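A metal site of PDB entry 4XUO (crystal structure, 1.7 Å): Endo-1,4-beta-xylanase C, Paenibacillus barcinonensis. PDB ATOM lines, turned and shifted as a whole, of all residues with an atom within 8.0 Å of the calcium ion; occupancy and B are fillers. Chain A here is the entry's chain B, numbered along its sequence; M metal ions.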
ATOM      1  N   HIS A  14     -11.875   4.528 -28.883  1.00  0.00           N
ATOM      2  CA  HIS A  14     -10.972   3.452 -28.536  1.00  0.00           C
ATOM      3  C   HIS A  14     -11.535   2.113 -28.970  1.00  0.00           C
ATOM      4  O   HIS A  14     -12.577   1.676 -28.414  1.00  0.00           O
ATOM      5  CB  HIS A  14     -10.738   3.421 -27.009  1.00  0.00           C
ATOM      6  CG  HIS A  14     -10.145   4.677 -26.463  1.00  0.00           C
ATOM      7  ND1 HIS A  14     -10.194   4.994 -25.133  1.00  0.00           N
ATOM      8  CD2 HIS A  14      -9.468   5.682 -27.062  1.00  0.00           C
ATOM      9  CE1 HIS A  14      -9.577   6.140 -24.919  1.00  0.00           C
ATOM     10  NE2 HIS A  14      -9.153   6.595 -26.087  1.00  0.00           N
ATOM     11  N   SER A  15     -10.880   1.479 -29.936  1.00  0.00           N
ATOM     12  CA  SER A  15     -11.226   0.141 -30.422  1.00  0.00           C
ATOM     13  C   SER A  15     -10.265  -0.971 -29.874  1.00  0.00           C
ATOM     14  O   SER A  15     -10.503  -2.148 -30.024  1.00  0.00           O
ATOM     15  CB  SER A  15     -11.247   0.124 -31.950  1.00  0.00           C
ATOM     16  OG  SER A  15     -12.268   1.000 -32.420  1.00  0.00           O
ATOM     17  N   PHE A  16      -9.184  -0.523 -29.239  1.00  0.00           N
ATOM     18  CA  PHE A  16      -8.216  -1.396 -28.575  1.00  0.00           C
ATOM     19  C   PHE A  16      -7.477  -2.367 -29.496  1.00  0.00           C
ATOM     20  O   PHE A  16      -7.086  -3.465 -29.055  1.00  0.00           O
ATOM     21  CB  PHE A  16      -8.921  -2.142 -27.419  1.00  0.00           C
ATOM     22  CG  PHE A  16      -9.564  -1.213 -26.419  1.00  0.00           C
ATOM     23  CD1 PHE A  16      -8.781  -0.436 -25.566  1.00  0.00           C
ATOM     24  CD2 PHE A  16     -10.960  -1.084 -26.312  1.00  0.00           C
ATOM     25  CE1 PHE A  16      -9.332   0.451 -24.668  1.00  0.00           C
ATOM     26  CE2 PHE A  16     -11.511  -0.203 -25.405  1.00  0.00           C
ATOM     27  CZ  PHE A  16     -10.708   0.570 -24.591  1.00  0.00           C
ATOM     28  N   GLU A  17      -7.267  -1.982 -30.762  1.00  0.00           N
ATOM     29  CA  GLU A  17      -6.773  -2.926 -31.755  1.00  0.00           C
ATOM     30  C   GLU A  17      -5.250  -2.999 -31.889  1.00  0.00           C
ATOM     31  O   GLU A  17      -4.758  -3.821 -32.674  1.00  0.00           O
ATOM     32  CB  GLU A  17      -7.357  -2.654 -33.131  1.00  0.00           C
ATOM     33  CG  GLU A  17      -8.864  -2.418 -33.155  1.00  0.00           C
ATOM     34  CD  GLU A  17      -9.719  -3.582 -32.771  1.00  0.00           C
ATOM     35  OE1 GLU A  17      -9.206  -4.678 -32.498  1.00  0.00           O
ATOM     36  OE2 GLU A  17     -10.969  -3.412 -32.713  1.00  0.00           O
ATOM     37  N   GLU A  18      -4.533  -2.209 -31.109  1.00  0.00           N
ATOM     38  CA  GLU A  18      -3.107  -2.214 -31.162  1.00  0.00           C
ATOM     39  C   GLU A  18      -2.398  -2.664 -29.855  1.00  0.00           C
ATOM     40  O   GLU A  18      -2.911  -3.482 -29.176  1.00  0.00           O
ATOM     41  CB  GLU A  18      -2.618  -0.881 -31.654  1.00  0.00           C
ATOM     42  CG  GLU A  18      -3.061  -0.624 -33.056  1.00  0.00           C
ATOM     43  CD  GLU A  18      -2.402   0.600 -33.646  1.00  0.00           C
ATOM     44  OE1 GLU A  18      -2.836   1.728 -33.368  1.00  0.00           O
ATOM     45  OE2 GLU A  18      -1.427   0.466 -34.374  1.00  0.00           O
ATOM     46  N   GLN A  22      -4.671   2.529 -24.701  1.00  0.00           N
ATOM     47  CA  GLN A  22      -5.145   3.875 -25.089  1.00  0.00           C
ATOM     48  C   GLN A  22      -5.532   4.785 -23.919  1.00  0.00           C
ATOM     49  O   GLN A  22      -6.528   5.504 -23.969  1.00  0.00           O
ATOM     50  CB  GLN A  22      -6.324   3.748 -26.135  1.00  0.00           C
ATOM     51  CG  GLN A  22      -5.931   2.815 -27.284  1.00  0.00           C
ATOM     52  CD  GLN A  22      -6.941   2.709 -28.451  1.00  0.00           C
ATOM     53  OE1 GLN A  22      -7.471   1.648 -28.708  1.00  0.00           O
ATOM     54  NE2 GLN A  22      -7.159   3.790 -29.168  1.00  0.00           N
ATOM     55  N   VAL A  34      -5.183  -5.252 -22.939  1.00  0.00           N
ATOM     56  CA  VAL A  34      -5.845  -5.646 -24.168  1.00  0.00           C
ATOM     57  C   VAL A  34      -5.857  -7.191 -24.273  1.00  0.00           C
ATOM     58  O   VAL A  34      -4.969  -7.863 -23.741  1.00  0.00           O
ATOM     59  CB  VAL A  34      -5.206  -5.001 -25.399  1.00  0.00           C
ATOM     60  CG1 VAL A  34      -5.912  -5.468 -26.649  1.00  0.00           C
ATOM     61  CG2 VAL A  34      -5.289  -3.477 -25.317  1.00  0.00           C
ATOM     62  N   THR A  35      -6.881  -7.760 -24.917  1.00  0.00           N
ATOM     63  CA  THR A  35      -7.007  -9.196 -25.139  1.00  0.00           C
ATOM     64  C   THR A  35      -7.471  -9.425 -26.565  1.00  0.00           C
ATOM     65  O   THR A  35      -8.201  -8.579 -27.122  1.00  0.00           O
ATOM     66  CB  THR A  35      -7.989  -9.875 -24.182  1.00  0.00           C
ATOM     67  OG1 THR A  35      -8.044 -11.276 -24.443  1.00  0.00           O
ATOM     68  CG2 THR A  35      -9.412  -9.295 -24.333  1.00  0.00           C
ATOM     69  N   GLN A  38     -11.492 -12.241 -27.231  1.00  0.00           N
ATOM     70  CA  GLN A  38     -12.822 -11.832 -27.683  1.00  0.00           C
ATOM     71  C   GLN A  38     -12.849 -10.346 -27.957  1.00  0.00           C
ATOM     72  O   GLN A  38     -12.013  -9.574 -27.453  1.00  0.00           O
ATOM     73  CB  GLN A  38     -13.867 -12.107 -26.621  1.00  0.00           C
ATOM     74  CG  GLN A  38     -14.149 -13.567 -26.369  1.00  0.00           C
ATOM     75  CD  GLN A  38     -15.087 -13.756 -25.195  1.00  0.00           C
ATOM     76  OE1 GLN A  38     -15.177 -12.902 -24.306  1.00  0.00           O
ATOM     77  NE2 GLN A  38     -15.780 -14.882 -25.182  1.00  0.00           N
ATOM     78  N   ALA A  39     -13.798  -9.924 -28.790  1.00  0.00           N
ATOM     79  CA  ALA A  39     -13.989  -8.502 -29.054  1.00  0.00           C
ATOM     80  C   ALA A  39     -15.383  -8.280 -29.588  1.00  0.00           C
ATOM     81  O   ALA A  39     -16.040  -9.246 -30.031  1.00  0.00           O
ATOM     82  CB  ALA A  39     -12.976  -7.989 -30.070  1.00  0.00           C
ATOM     83  N   TYR A  40     -15.844  -7.033 -29.494  1.00  0.00           N
ATOM     84  CA  TYR A  40     -17.150  -6.644 -30.077  1.00  0.00           C
ATOM     85  C   TYR A  40     -16.984  -6.428 -31.557  1.00  0.00           C
ATOM     86  O   TYR A  40     -17.789  -6.909 -32.363  1.00  0.00           O
ATOM     87  CB  TYR A  40     -17.703  -5.379 -29.424  1.00  0.00           C
ATOM     88  CG  TYR A  40     -19.078  -5.046 -29.935  1.00  0.00           C
ATOM     89  CD1 TYR A  40     -20.143  -5.891 -29.686  1.00  0.00           C
ATOM     90  CD2 TYR A  40     -19.304  -3.904 -30.672  1.00  0.00           C
ATOM     91  CE1 TYR A  40     -21.414  -5.604 -30.145  1.00  0.00           C
ATOM     92  CE2 TYR A  40     -20.572  -3.608 -31.162  1.00  0.00           C
ATOM     93  CZ  TYR A  40     -21.614  -4.470 -30.889  1.00  0.00           C
ATOM     94  OH  TYR A  40     -22.910  -4.190 -31.376  1.00  0.00           O
ATOM     95  N   GLN A  41     -15.970  -5.664 -31.939  1.00  0.00           N
ATOM     96  CA  GLN A  41     -15.533  -5.615 -33.330  1.00  0.00           C
ATOM     97  C   GLN A  41     -14.019  -5.498 -33.343  1.00  0.00           C
ATOM     98  O   GLN A  41     -13.380  -5.206 -32.296  1.00  0.00           O
ATOM     99  CB  GLN A  41     -16.230  -4.529 -34.210  1.00  0.00           C
ATOM    100  CG  GLN A  41     -15.923  -3.079 -33.888  1.00  0.00           C
ATOM    101  CD  GLN A  41     -16.025  -2.087 -35.056  1.00  0.00           C
ATOM    102  OE1 GLN A  41     -15.489  -0.966 -34.985  1.00  0.00           O
ATOM    103  NE2 GLN A  41     -16.673  -2.499 -36.107  1.00  0.00           N
ATOM    104  N   GLY A  42     -13.448  -5.761 -34.509  1.00  0.00           N
ATOM    105  CA  GLY A  42     -11.992  -6.037 -34.640  1.00  0.00           C
ATOM    106  C   GLY A  42     -11.607  -7.308 -33.858  1.00  0.00           C
ATOM    107  O   GLY A  42     -12.452  -8.045 -33.345  1.00  0.00           O
ATOM    108  N   LYS A  43     -10.306  -7.504 -33.756  1.00  0.00           N
ATOM    109  CA  LYS A  43      -9.712  -8.632 -33.032  1.00  0.00           C
ATOM    110  C   LYS A  43      -9.692  -8.490 -31.519  1.00  0.00           C
ATOM    111  O   LYS A  43      -9.795  -9.516 -30.817  1.00  0.00           O
ATOM    112  CB  LYS A  43      -8.266  -8.818 -33.531  1.00  0.00           C
ATOM    113  CG  LYS A  43      -7.519 -10.032 -32.972  1.00  0.00           C
ATOM    114  CD  LYS A  43      -8.061 -11.335 -33.526  1.00  0.00           C
ATOM    115  CE  LYS A  43      -7.362 -12.532 -32.871  1.00  0.00           C
ATOM    116  NZ  LYS A  43      -7.146 -13.655 -33.828  1.00  0.00           N
ATOM    117  N   GLN A  44      -9.550  -7.257 -31.011  1.00  0.00           N
ATOM    118  CA  GLN A  44      -9.200  -7.020 -29.625  1.00  0.00           C
ATOM    119  C   GLN A  44     -10.193  -6.116 -28.881  1.00  0.00           C
ATOM    120  O   GLN A  44     -10.844  -5.250 -29.487  1.00  0.00           O
ATOM    121  CB  GLN A  44      -7.809  -6.380 -29.563  1.00  0.00           C
ATOM    122  CG  GLN A  44      -6.716  -7.261 -30.104  1.00  0.00           C
ATOM    123  CD  GLN A  44      -5.312  -6.677 -30.007  1.00  0.00           C
ATOM    124  OE1 GLN A  44      -5.090  -5.490 -29.744  1.00  0.00           O
ATOM    125  NE2 GLN A  44      -4.326  -7.538 -30.225  1.00  0.00           N
ATOM    126  N   SER A  45     -10.254  -6.322 -27.553  1.00  0.00           N
ATOM    127  CA  SER A  45     -11.001  -5.487 -26.610  1.00  0.00           C
ATOM    128  C   SER A  45     -10.139  -5.283 -25.330  1.00  0.00           C
ATOM    129  O   SER A  45      -8.999  -5.779 -25.272  1.00  0.00           O
ATOM    130  CB  SER A  45     -12.359  -6.149 -26.273  1.00  0.00           C
ATOM    131  OG  SER A  45     -12.165  -7.411 -25.635  1.00  0.00           O
ATOM    132  N   LEU A  46     -10.683  -4.574 -24.355  1.00  0.00           N
ATOM    133  CA  LEU A  46      -9.991  -4.264 -23.073  1.00  0.00           C
ATOM    134  C   LEU A  46     -10.552  -5.137 -21.967  1.00  0.00           C
ATOM    135  O   LEU A  46     -11.749  -5.026 -21.639  1.00  0.00           O
ATOM    136  CB  LEU A  46     -10.201  -2.802 -22.695  1.00  0.00           C
ATOM    137  CG  LEU A  46      -9.388  -2.326 -21.454  1.00  0.00           C
ATOM    138  CD1 LEU A  46      -7.954  -2.118 -21.869  1.00  0.00           C
ATOM    139  CD2 LEU A  46      -9.976  -1.075 -20.867  1.00  0.00           C
ATOM    140  N   TRP A 118     -22.809  -9.057 -25.678  1.00  0.00           N
ATOM    141  CA  TRP A 118     -22.344  -7.693 -25.439  1.00  0.00           C
ATOM    142  C   TRP A 118     -23.529  -6.743 -25.255  1.00  0.00           C
ATOM    143  O   TRP A 118     -24.530  -6.814 -26.008  1.00  0.00           O
ATOM    144  CB  TRP A 118     -21.460  -7.166 -26.597  1.00  0.00           C
ATOM    145  CG  TRP A 118     -20.145  -7.896 -26.800  1.00  0.00           C
ATOM    146  CD1 TRP A 118     -19.950  -9.029 -27.537  1.00  0.00           C
ATOM    147  CD2 TRP A 118     -18.855  -7.520 -26.310  1.00  0.00           C
ATOM    148  NE1 TRP A 118     -18.623  -9.402 -27.501  1.00  0.00           N
ATOM    149  CE2 TRP A 118     -17.930  -8.498 -26.755  1.00  0.00           C
ATOM    150  CE3 TRP A 118     -18.395  -6.460 -25.506  1.00  0.00           C
ATOM    151  CZ2 TRP A 118     -16.563  -8.439 -26.434  1.00  0.00           C
ATOM    152  CZ3 TRP A 118     -17.033  -6.413 -25.192  1.00  0.00           C
ATOM    153  CH2 TRP A 118     -16.150  -7.387 -25.656  1.00  0.00           C
ATOM    154  N   LEU A 148     -14.449  -4.430 -22.054  1.00  0.00           N
ATOM    155  CA  LEU A 148     -14.960  -3.188 -22.649  1.00  0.00           C
ATOM    156  C   LEU A 148     -14.433  -3.061 -24.088  1.00  0.00           C
ATOM    157  O   LEU A 148     -13.268  -3.297 -24.352  1.00  0.00           O
ATOM    158  CB  LEU A 148     -14.530  -1.962 -21.845  1.00  0.00           C
ATOM    159  CG  LEU A 148     -14.704  -0.553 -22.474  1.00  0.00           C
ATOM    160  CD1 LEU A 148     -16.187  -0.238 -22.543  1.00  0.00           C
ATOM    161  CD2 LEU A 148     -14.031   0.534 -21.646  1.00  0.00           C
ATOM    162  N   ASP A 149     -15.290  -2.648 -25.036  1.00  0.00           N
ATOM    163  CA  ASP A 149     -14.791  -2.444 -26.377  1.00  0.00           C
ATOM    164  C   ASP A 149     -15.560  -1.311 -27.047  1.00  0.00           C
ATOM    165  O   ASP A 149     -16.653  -0.949 -26.622  1.00  0.00           O
ATOM    166  CB  ASP A 149     -14.898  -3.734 -27.207  1.00  0.00           C
ATOM    167  CG  ASP A 149     -13.970  -3.764 -28.412  1.00  0.00           C
ATOM    168  OD1 ASP A 149     -13.013  -2.936 -28.479  1.00  0.00           O
ATOM    169  OD2 ASP A 149     -14.126  -4.632 -29.292  1.00  0.00           O
ATOM    170  N   GLU A 150     -14.932  -0.753 -28.072  1.00  0.00           N
ATOM    171  CA  GLU A 150     -15.545   0.266 -28.925  1.00  0.00           C
ATOM    172  C   GLU A 150     -16.088   1.424 -28.079  1.00  0.00           C
ATOM    173  O   GLU A 150     -17.268   1.799 -28.142  1.00  0.00           O
ATOM    174  CB  GLU A 150     -16.584  -0.392 -29.802  1.00  0.00           C
ATOM    175  CG  GLU A 150     -16.027  -1.479 -30.686  1.00  0.00           C
ATOM    176  CD  GLU A 150     -14.741  -1.102 -31.417  1.00  0.00           C
ATOM    177  OE1 GLU A 150     -14.763  -0.091 -32.172  1.00  0.00           O
ATOM    178  OE2 GLU A 150     -13.726  -1.847 -31.312  1.00  0.00           O
ATOM    179  N   PHE A 151     -15.178   1.986 -27.295  1.00  0.00           N
ATOM    180  CA  PHE A 151     -15.502   3.087 -26.409  1.00  0.00           C
ATOM    181  C   PHE A 151     -15.504   4.381 -27.186  1.00  0.00           C
ATOM    182  O   PHE A 151     -14.608   4.611 -27.976  1.00  0.00           O
ATOM    183  CB  PHE A 151     -14.475   3.175 -25.242  1.00  0.00           C
ATOM    184  CG  PHE A 151     -14.727   4.319 -24.306  1.00  0.00           C
ATOM    185  CD1 PHE A 151     -15.792   4.298 -23.390  1.00  0.00           C
ATOM    186  CD2 PHE A 151     -13.931   5.442 -24.336  1.00  0.00           C
ATOM    187  CE1 PHE A 151     -16.024   5.384 -22.551  1.00  0.00           C
ATOM    188  CE2 PHE A 151     -14.151   6.500 -23.503  1.00  0.00           C
ATOM    189  CZ  PHE A 151     -15.195   6.494 -22.613  1.00  0.00           C
HETATM  190 CA    CA M   1     -12.176  -3.772 -30.728  1.00  0.00          CA
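OE1 of Gln 44 lies close to O of Phe 16 (2.9 Å). The side-chain amide oxygen (OE1) of Gln 44 lies close to the backbone carbonyl oxygen (O) of Glu 18. OE1 of Glu 17 lies within hydrogen-bond range of N of Lys 43 (3.3 Å). The backbone carbonyl oxygen (O) of His 14 lies close to the backbone NH (N) of Glu 150, 3.4 Å away. The backbone NH (N) of Tyr 40 sits close to the side-chain carboxylate (OD2) of Asp 149 (3.0 Å).
Within 4 Å of the calcium ion: Ser 15, Glu 17, Gln 41, Gln 44, Asp 149 and Glu 150. The nearest printed residue that does not touch the calcium ion is Ala 39 (4.3 Å).
The calcium ion is bound by O of Gln 44 (2.3 Å), OE2 of Glu 17 (2.4 Å), O of Ser 15 (2.4 Å), O of Gln 41 (2.4 Å), OE2 of Glu 150 (2.5 Å), OD1 of Asp 149 (2.5 Å) and OD2 of Asp 149 (2.6 Å). The calcium ion has seven donor atoms within binding distance.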
